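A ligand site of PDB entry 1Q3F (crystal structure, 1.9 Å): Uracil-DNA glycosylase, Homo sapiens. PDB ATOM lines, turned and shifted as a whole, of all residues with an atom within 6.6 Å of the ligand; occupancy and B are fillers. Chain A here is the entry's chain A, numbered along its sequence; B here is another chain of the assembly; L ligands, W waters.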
ATOM      1  N   LEU A  61     -11.969  31.235  -2.921  1.00  0.00           N
ATOM      2  CA  LEU A  61     -12.533  29.937  -3.275  1.00  0.00           C
ATOM      3  C   LEU A  61     -11.519  29.122  -4.072  1.00  0.00           C
ATOM      4  O   LEU A  61     -11.060  29.552  -5.127  1.00  0.00           O
ATOM      5  CB  LEU A  61     -13.815  30.117  -4.109  1.00  0.00           C
ATOM      6  CG  LEU A  61     -15.104  29.300  -3.894  1.00  0.00           C
ATOM      7  CD1 LEU A  61     -15.818  29.169  -5.225  1.00  0.00           C
ATOM      8  CD2 LEU A  61     -14.838  27.943  -3.335  1.00  0.00           C
ATOM      9  N   GLY A  62     -11.181  27.950  -3.544  1.00  0.00           N
ATOM     10  CA  GLY A  62     -10.256  27.050  -4.206  1.00  0.00           C
ATOM     11  C   GLY A  62     -11.070  25.895  -4.765  1.00  0.00           C
ATOM     12  O   GLY A  62     -12.304  25.926  -4.749  1.00  0.00           O
ATOM     13  N   GLN A  63     -10.368  24.860  -5.234  1.00  0.00           N
ATOM     14  CA  GLN A  63     -11.007  23.684  -5.834  1.00  0.00           C
ATOM     15  C   GLN A  63     -11.448  22.616  -4.835  1.00  0.00           C
ATOM     16  O   GLN A  63     -12.640  22.348  -4.672  1.00  0.00           O
ATOM     17  CB  GLN A  63     -10.036  23.068  -6.865  1.00  0.00           C
ATOM     18  CG  GLN A  63     -10.521  21.783  -7.503  1.00  0.00           C
ATOM     19  CD  GLN A  63      -9.465  21.177  -8.415  1.00  0.00           C
ATOM     20  OE1 GLN A  63      -9.115  21.749  -9.449  1.00  0.00           O
ATOM     21  NE2 GLN A  63      -8.937  20.018  -8.029  1.00  0.00           N
ATOM     22  N   ASP A  64     -10.479  21.980  -4.178  1.00  0.00           N
ATOM     23  CA  ASP A  64     -10.764  20.949  -3.191  1.00  0.00           C
ATOM     24  C   ASP A  64      -9.554  20.838  -2.265  1.00  0.00           C
ATOM     25  O   ASP A  64      -8.461  21.268  -2.632  1.00  0.00           O
ATOM     26  CB  ASP A  64     -11.101  19.611  -3.871  1.00  0.00           C
ATOM     27  CG  ASP A  64      -9.914  18.973  -4.576  1.00  0.00           C
ATOM     28  OD1 ASP A  64      -9.773  17.739  -4.426  1.00  0.00           O
ATOM     29  OD2 ASP A  64      -9.148  19.676  -5.277  1.00  0.00           O
ATOM     30  N   PRO A  65      -9.721  20.235  -1.075  1.00  0.00           N
ATOM     31  CA  PRO A  65      -8.648  20.077  -0.070  1.00  0.00           C
ATOM     32  C   PRO A  65      -7.319  19.417  -0.456  1.00  0.00           C
ATOM     33  O   PRO A  65      -7.210  18.717  -1.458  1.00  0.00           O
ATOM     34  CB  PRO A  65      -9.329  19.282   1.054  1.00  0.00           C
ATOM     35  CG  PRO A  65     -10.800  19.560   0.853  1.00  0.00           C
ATOM     36  CD  PRO A  65     -10.924  19.498  -0.645  1.00  0.00           C
ATOM     37  N   TYR A  66      -6.308  19.675   0.380  1.00  0.00           N
ATOM     38  CA  TYR A  66      -5.010  19.068   0.188  1.00  0.00           C
ATOM     39  C   TYR A  66      -5.333  17.577   0.370  1.00  0.00           C
ATOM     40  O   TYR A  66      -6.157  17.209   1.216  1.00  0.00           O
ATOM     41  CB  TYR A  66      -4.023  19.538   1.272  1.00  0.00           C
ATOM     42  CG  TYR A  66      -3.476  20.920   1.050  1.00  0.00           C
ATOM     43  CD1 TYR A  66      -2.696  21.214  -0.069  1.00  0.00           C
ATOM     44  CD2 TYR A  66      -3.694  21.940   1.984  1.00  0.00           C
ATOM     45  CE1 TYR A  66      -2.155  22.492  -0.260  1.00  0.00           C
ATOM     46  CE2 TYR A  66      -3.162  23.213   1.807  1.00  0.00           C
ATOM     47  CZ  TYR A  66      -2.394  23.489   0.681  1.00  0.00           C
ATOM     48  OH  TYR A  66      -1.870  24.754   0.496  1.00  0.00           O
ATOM     49  N   ALA A  72      -4.845  19.152   4.868  1.00  0.00           N
ATOM     50  CA  ALA A  72      -6.129  19.856   4.930  1.00  0.00           C
ATOM     51  C   ALA A  72      -6.762  19.864   6.314  1.00  0.00           C
ATOM     52  O   ALA A  72      -6.766  18.851   7.010  1.00  0.00           O
ATOM     53  CB  ALA A  72      -7.107  19.250   3.935  1.00  0.00           C
ATOM     54  N   LEU A  75      -9.806  24.933   6.069  1.00  0.00           N
ATOM     55  CA  LEU A  75      -9.600  26.277   5.554  1.00  0.00           C
ATOM     56  C   LEU A  75      -8.799  26.061   4.275  1.00  0.00           C
ATOM     57  O   LEU A  75      -7.753  25.415   4.320  1.00  0.00           O
ATOM     58  CB  LEU A  75      -8.803  27.133   6.546  1.00  0.00           C
ATOM     59  CG  LEU A  75      -9.384  27.320   7.947  1.00  0.00           C
ATOM     60  CD1 LEU A  75      -8.459  28.204   8.767  1.00  0.00           C
ATOM     61  CD2 LEU A  75     -10.786  27.934   7.847  1.00  0.00           C
ATOM     62  N   CYS A  76      -9.268  26.601   3.150  1.00  0.00           N
ATOM     63  CA  CYS A  76      -8.563  26.388   1.895  1.00  0.00           C
ATOM     64  C   CYS A  76      -7.119  26.864   1.903  1.00  0.00           C
ATOM     65  O   CYS A  76      -6.809  27.946   2.416  1.00  0.00           O
ATOM     66  CB  CYS A  76      -9.341  27.031   0.724  1.00  0.00           C
ATOM     67  SG  CYS A  76      -9.321  28.845   0.649  1.00  0.00           S
ATOM     68  N   PHE A  77      -6.230  26.028   1.341  1.00  0.00           N
ATOM     69  CA  PHE A  77      -4.800  26.292   1.220  1.00  0.00           C
ATOM     70  C   PHE A  77      -3.981  26.326   2.522  1.00  0.00           C
ATOM     71  O   PHE A  77      -2.749  26.448   2.480  1.00  0.00           O
ATOM     72  CB  PHE A  77      -4.586  27.585   0.446  1.00  0.00           C
ATOM     73  CG  PHE A  77      -5.170  27.555  -0.929  1.00  0.00           C
ATOM     74  CD1 PHE A  77      -4.595  26.762  -1.920  1.00  0.00           C
ATOM     75  CD2 PHE A  77      -6.323  28.261  -1.221  1.00  0.00           C
ATOM     76  CE1 PHE A  77      -5.155  26.679  -3.188  1.00  0.00           C
ATOM     77  CE2 PHE A  77      -6.891  28.183  -2.486  1.00  0.00           C
ATOM     78  CZ  PHE A  77      -6.313  27.389  -3.468  1.00  0.00           C
ATOM     79  N   SER A  78      -4.675  26.193   3.648  1.00  0.00           N
ATOM     80  CA  SER A  78      -4.041  26.225   4.962  1.00  0.00           C
ATOM     81  C   SER A  78      -3.619  24.861   5.508  1.00  0.00           C
ATOM     82  O   SER A  78      -4.209  23.821   5.170  1.00  0.00           O
ATOM     83  CB  SER A  78      -5.021  26.905   5.946  1.00  0.00           C
ATOM     84  OG  SER A  78      -4.498  26.991   7.270  1.00  0.00           O
ATOM     85  N   SER A  88       1.019  24.545  -3.279  1.00  0.00           N
ATOM     86  CA  SER A  88       0.069  25.614  -3.560  1.00  0.00           C
ATOM     87  C   SER A  88       0.243  26.833  -2.676  1.00  0.00           C
ATOM     88  O   SER A  88       0.206  27.961  -3.163  1.00  0.00           O
ATOM     89  CB  SER A  88      -1.371  25.103  -3.410  1.00  0.00           C
ATOM     90  OG  SER A  88      -1.685  24.154  -4.407  1.00  0.00           O
ATOM     91  N   LEU A  89       0.432  26.614  -1.379  1.00  0.00           N
ATOM     92  CA  LEU A  89       0.593  27.715  -0.430  1.00  0.00           C
ATOM     93  C   LEU A  89       1.927  28.441  -0.589  1.00  0.00           C
ATOM     94  O   LEU A  89       1.991  29.652  -0.377  1.00  0.00           O
ATOM     95  CB  LEU A  89       0.436  27.222   1.015  1.00  0.00           C
ATOM     96  CG  LEU A  89       0.545  28.279   2.109  1.00  0.00           C
ATOM     97  CD1 LEU A  89      -0.414  29.428   1.823  1.00  0.00           C
ATOM     98  CD2 LEU A  89       0.242  27.653   3.474  1.00  0.00           C
ATOM     99  N   LEU A 122     -12.786  29.106   1.583  1.00  0.00           N
ATOM    100  CA  LEU A 122     -13.627  28.029   1.099  1.00  0.00           C
ATOM    101  C   LEU A 122     -13.102  27.314  -0.137  1.00  0.00           C
ATOM    102  O   LEU A 122     -12.299  27.871  -0.886  1.00  0.00           O
ATOM    103  CB  LEU A 122     -15.011  28.605   0.780  1.00  0.00           C
ATOM    104  CG  LEU A 122     -16.174  27.660   0.489  1.00  0.00           C
ATOM    105  CD1 LEU A 122     -16.672  27.004   1.786  1.00  0.00           C
ATOM    106  CD2 LEU A 122     -17.300  28.448  -0.161  1.00  0.00           C
ATOM    107  N   ASN A 123     -13.534  26.069  -0.303  1.00  0.00           N
ATOM    108  CA  ASN A 123     -13.220  25.239  -1.467  1.00  0.00           C
ATOM    109  C   ASN A 123     -14.584  24.866  -2.074  1.00  0.00           C
ATOM    110  O   ASN A 123     -15.579  24.762  -1.351  1.00  0.00           O
ATOM    111  CB  ASN A 123     -12.494  23.934  -1.081  1.00  0.00           C
ATOM    112  CG  ASN A 123     -10.993  24.105  -0.911  1.00  0.00           C
ATOM    113  OD1 ASN A 123     -10.334  24.778  -1.701  1.00  0.00           O
ATOM    114  ND2 ASN A 123     -10.446  23.483   0.120  1.00  0.00           N
ATOM    115  N   TRP A 164     -10.056  31.077  -7.674  1.00  0.00           N
ATOM    116  CA  TRP A 164      -8.818  30.519  -8.194  1.00  0.00           C
ATOM    117  C   TRP A 164      -9.049  29.150  -8.828  1.00  0.00           C
ATOM    118  O   TRP A 164      -9.336  28.180  -8.125  1.00  0.00           O
ATOM    119  CB  TRP A 164      -7.780  30.438  -7.068  1.00  0.00           C
ATOM    120  CG  TRP A 164      -7.422  31.782  -6.438  1.00  0.00           C
ATOM    121  CD1 TRP A 164      -7.662  33.021  -6.956  1.00  0.00           C
ATOM    122  CD2 TRP A 164      -6.704  31.996  -5.212  1.00  0.00           C
ATOM    123  NE1 TRP A 164      -7.121  33.994  -6.146  1.00  0.00           N
ATOM    124  CE2 TRP A 164      -6.525  33.388  -5.068  1.00  0.00           C
ATOM    125  CE3 TRP A 164      -6.182  31.134  -4.232  1.00  0.00           C
ATOM    126  CZ2 TRP A 164      -5.846  33.946  -3.979  1.00  0.00           C
ATOM    127  CZ3 TRP A 164      -5.506  31.692  -3.151  1.00  0.00           C
ATOM    128  CH2 TRP A 164      -5.350  33.081  -3.032  1.00  0.00           C
ATOM    129  N   HIS A 187      -5.354  28.563 -10.702  1.00  0.00           N
ATOM    130  CA  HIS A 187      -5.157  27.932  -9.387  1.00  0.00           C
ATOM    131  C   HIS A 187      -3.654  28.017  -9.028  1.00  0.00           C
ATOM    132  O   HIS A 187      -2.796  27.866  -9.891  1.00  0.00           O
ATOM    133  CB  HIS A 187      -5.652  26.483  -9.473  1.00  0.00           C
ATOM    134  CG  HIS A 187      -5.730  25.792  -8.146  1.00  0.00           C
ATOM    135  ND1 HIS A 187      -4.613  25.273  -7.507  1.00  0.00           N
ATOM    136  CD2 HIS A 187      -6.781  25.537  -7.333  1.00  0.00           C
ATOM    137  CE1 HIS A 187      -4.989  24.729  -6.358  1.00  0.00           C
ATOM    138  NE2 HIS A 187      -6.289  24.872  -6.230  1.00  0.00           N
ATOM    139  N   PRO A 188      -3.329  28.278  -7.746  1.00  0.00           N
ATOM    140  CA  PRO A 188      -1.916  28.379  -7.334  1.00  0.00           C
ATOM    141  C   PRO A 188      -1.075  27.089  -7.328  1.00  0.00           C
ATOM    142  O   PRO A 188       0.129  27.122  -7.066  1.00  0.00           O
ATOM    143  CB  PRO A 188      -2.014  29.037  -5.954  1.00  0.00           C
ATOM    144  CG  PRO A 188      -3.344  28.561  -5.429  1.00  0.00           C
ATOM    145  CD  PRO A 188      -4.231  28.659  -6.650  1.00  0.00           C
ATOM    146  N   SER A 189      -1.705  25.963  -7.622  1.00  0.00           N
ATOM    147  CA  SER A 189      -0.966  24.701  -7.675  1.00  0.00           C
ATOM    148  C   SER A 189       0.121  24.803  -8.751  1.00  0.00           C
ATOM    149  O   SER A 189      -0.077  25.462  -9.788  1.00  0.00           O
ATOM    150  CB  SER A 189      -1.916  23.539  -8.016  1.00  0.00           C
ATOM    151  OG  SER A 189      -1.173  22.361  -8.334  1.00  0.00           O
ATOM    152  P    DT B   3       1.254  14.560  -5.022  1.00  0.00           P
ATOM    153  OP1  DT B   3       0.987  13.957  -3.690  1.00  0.00           O
ATOM    154  OP2  DT B   3       0.584  13.992  -6.232  1.00  0.00           O
ATOM    155  O5'  DT B   3       0.912  16.114  -4.975  1.00  0.00           O
ATOM    156  C5'  DT B   3       1.701  17.012  -4.191  1.00  0.00           C
ATOM    157  C4'  DT B   3       1.680  18.393  -4.795  1.00  0.00           C
ATOM    158  O4'  DT B   3       2.514  18.443  -5.972  1.00  0.00           O
ATOM    159  C3'  DT B   3       0.300  18.919  -5.223  1.00  0.00           C
ATOM    160  O3'  DT B   3       0.141  20.281  -4.833  1.00  0.00           O
ATOM    161  C2'  DT B   3       0.333  18.828  -6.735  1.00  0.00           C
ATOM    162  C1'  DT B   3       1.811  19.043  -7.043  1.00  0.00           C
ATOM    163  N1   DT B   3       2.262  18.405  -8.294  1.00  0.00           N
ATOM    164  C2   DT B   3       3.191  19.066  -9.074  1.00  0.00           C
ATOM    165  O2   DT B   3       3.641  20.164  -8.781  1.00  0.00           O
ATOM    166  N3   DT B   3       3.564  18.401 -10.213  1.00  0.00           N
ATOM    167  C4   DT B   3       3.121  17.168 -10.651  1.00  0.00           C
ATOM    168  O4   DT B   3       3.552  16.689 -11.699  1.00  0.00           O
ATOM    169  C5   DT B   3       2.145  16.518  -9.790  1.00  0.00           C
ATOM    170  C7   DT B   3       1.600  15.185 -10.173  1.00  0.00           C
ATOM    171  C6   DT B   3       1.766  17.161  -8.671  1.00  0.00           C
ATOM    172  P   NRI B   4      -0.677  20.634  -3.502  1.00  0.00           P
ATOM    173  O1P NRI B   4      -0.577  22.105  -3.296  1.00  0.00           O
ATOM    174  O2P NRI B   4      -0.207  19.720  -2.430  1.00  0.00           O
ATOM    175  O5' NRI B   4      -2.190  20.213  -3.834  1.00  0.00           O
ATOM    176  C2' NRI B   4      -6.286  21.314  -5.520  1.00  0.00           C
ATOM    177  C5' NRI B   4      -2.984  20.926  -4.796  1.00  0.00           C
ATOM    178  C4' NRI B   4      -4.196  20.221  -5.041  1.00  0.00           C
ATOM    179  C3' NRI B   4      -4.983  20.904  -6.197  1.00  0.00           C
ATOM    180  C6' NRI B   4      -5.165  20.367  -3.863  1.00  0.00           C
ATOM    181  N1' NRI B   4      -6.430  20.186  -4.596  1.00  0.00           N
ATOM    182  O3' NRI B   4      -5.191  19.994  -7.284  1.00  0.00           O
ATOM    183  P    DA B   5      -4.167  20.011  -8.540  1.00  0.00           P
ATOM    184  OP1  DA B   5      -4.663  19.045  -9.558  1.00  0.00           O
ATOM    185  OP2  DA B   5      -2.788  19.880  -7.994  1.00  0.00           O
ATOM    186  O5'  DA B   5      -4.282  21.481  -9.139  1.00  0.00           O
ATOM    187  C5'  DA B   5      -5.400  21.871  -9.920  1.00  0.00           C
ATOM    188  C4'  DA B   5      -4.974  22.846 -10.991  1.00  0.00           C
ATOM    189  O4'  DA B   5      -3.924  22.238 -11.785  1.00  0.00           O
ATOM    190  C3'  DA B   5      -6.065  23.250 -11.972  1.00  0.00           C
ATOM    191  O3'  DA B   5      -5.817  24.600 -12.385  1.00  0.00           O
ATOM    192  C2'  DA B   5      -5.871  22.268 -13.118  1.00  0.00           C
ATOM    193  C1'  DA B   5      -4.359  22.054 -13.121  1.00  0.00           C
ATOM    194  N9   DA B   5      -3.906  20.730 -13.541  1.00  0.00           N
ATOM    195  C8   DA B   5      -3.998  19.573 -12.817  1.00  0.00           C
ATOM    196  N7   DA B   5      -3.466  18.532 -13.417  1.00  0.00           N
ATOM    197  C5   DA B   5      -3.011  19.042 -14.628  1.00  0.00           C
ATOM    198  C6   DA B   5      -2.340  18.435 -15.711  1.00  0.00           C
ATOM    199  N6   DA B   5      -1.990  17.145 -15.754  1.00  0.00           N
ATOM    200  N1   DA B   5      -2.025  19.222 -16.758  1.00  0.00           N
ATOM    201  C2   DA B   5      -2.362  20.517 -16.720  1.00  0.00           C
ATOM    202  N3   DA B   5      -2.983  21.194 -15.758  1.00  0.00           N
ATOM    203  C4   DA B   5      -3.288  20.390 -14.726  1.00  0.00           C
HETATM  204  N1  LIG L   1      -5.856  23.620  -3.317  1.00  0.00           N
HETATM  205  C1  LIG L   1      -7.196  23.919  -3.161  1.00  0.00           C
HETATM  206  O1  LIG L   1      -7.941  24.135  -4.100  1.00  0.00           O
HETATM  207  N2  LIG L   1      -7.643  23.952  -1.854  1.00  0.00           N
HETATM  208  C2  LIG L   1      -6.896  23.686  -0.715  1.00  0.00           C
HETATM  209  O2  LIG L   1      -7.434  23.755   0.392  1.00  0.00           O
HETATM  210  C3  LIG L   1      -5.520  23.367  -0.970  1.00  0.00           C
HETATM  211  C4  LIG L   1      -5.061  23.346  -2.228  1.00  0.00           C
HETATM  212  O   HOH W   1      -7.134  22.047   2.140  1.00  0.00           O
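The backbone NH of Phe 77 sits at hydrogen-bond distance from an oxygen (O2) of the ligand, at 2.7 Å. O1 of the ligand is in hydrogen-bond range of N of Gln 63 (2.8 Å). O1 of the ligand sits at hydrogen-bond distance from NE2 of His 187, at 2.8 Å. The side-chain amide oxygen of Asn 123 lies within hydrogen-bond range of a nitrogen (N2) of the ligand (2.8 Å). O1 of the ligand lies within hydrogen-bond range of N of Asp 64 (3.3 Å). The backbone carbonyl oxygen (O) of Asp 64 is in hydrogen-bond range of a nitrogen (N2) of the ligand (2.9 Å).
The side-chain hydroxyl (OH) of Tyr 66 is in hydrogen-bond range of the backbone carbonyl oxygen (O) of Phe 77 (2.8 Å). NE2 of Gln 63 sits at hydrogen-bond distance from OD2 of Asp 64, at 2.8 Å. A ring nitrogen (ND1) of His 187 sits at hydrogen-bond distance from the backbone NH (N) of Ser 189, 3.0 Å away. OG of Ser 88 is in hydrogen-bond range of O1P of NRI 4 of chain B, 2.6 Å away. O of Leu 122 lies close to SG of Cys 76 (3.5 Å). N of Gly 62 lies within hydrogen-bond range of O of Leu 122 (2.9 Å).
Merely in contact with the ligand: Gly 62 (3.7 Å), Pro 65 (3.9 Å), Tyr 66 (3.5 Å), Cys 76 (3.2 Å) and NRI 4 of chain B (3.2 Å). Hydrophobic or aromatic side chains that line the ligand: Tyr 66, Phe 77 and His 187. Ten residues have an atom within 4 Å of the ligand: Gly 62, Gln 63, Asp 64, Pro 65, Tyr 66, Cys 76, Phe 77, Asn 123, His 187 and NRI 4 of chain B. Along chain A the residues within 4 Å of the ligand span positions 62 to 187. The nearest printed residue that does not touch the ligand is Ser 88 (4.1 Å).
Water W1 bridges an oxygen (O2) of the ligand and the backbone NH (N) of Tyr 66.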
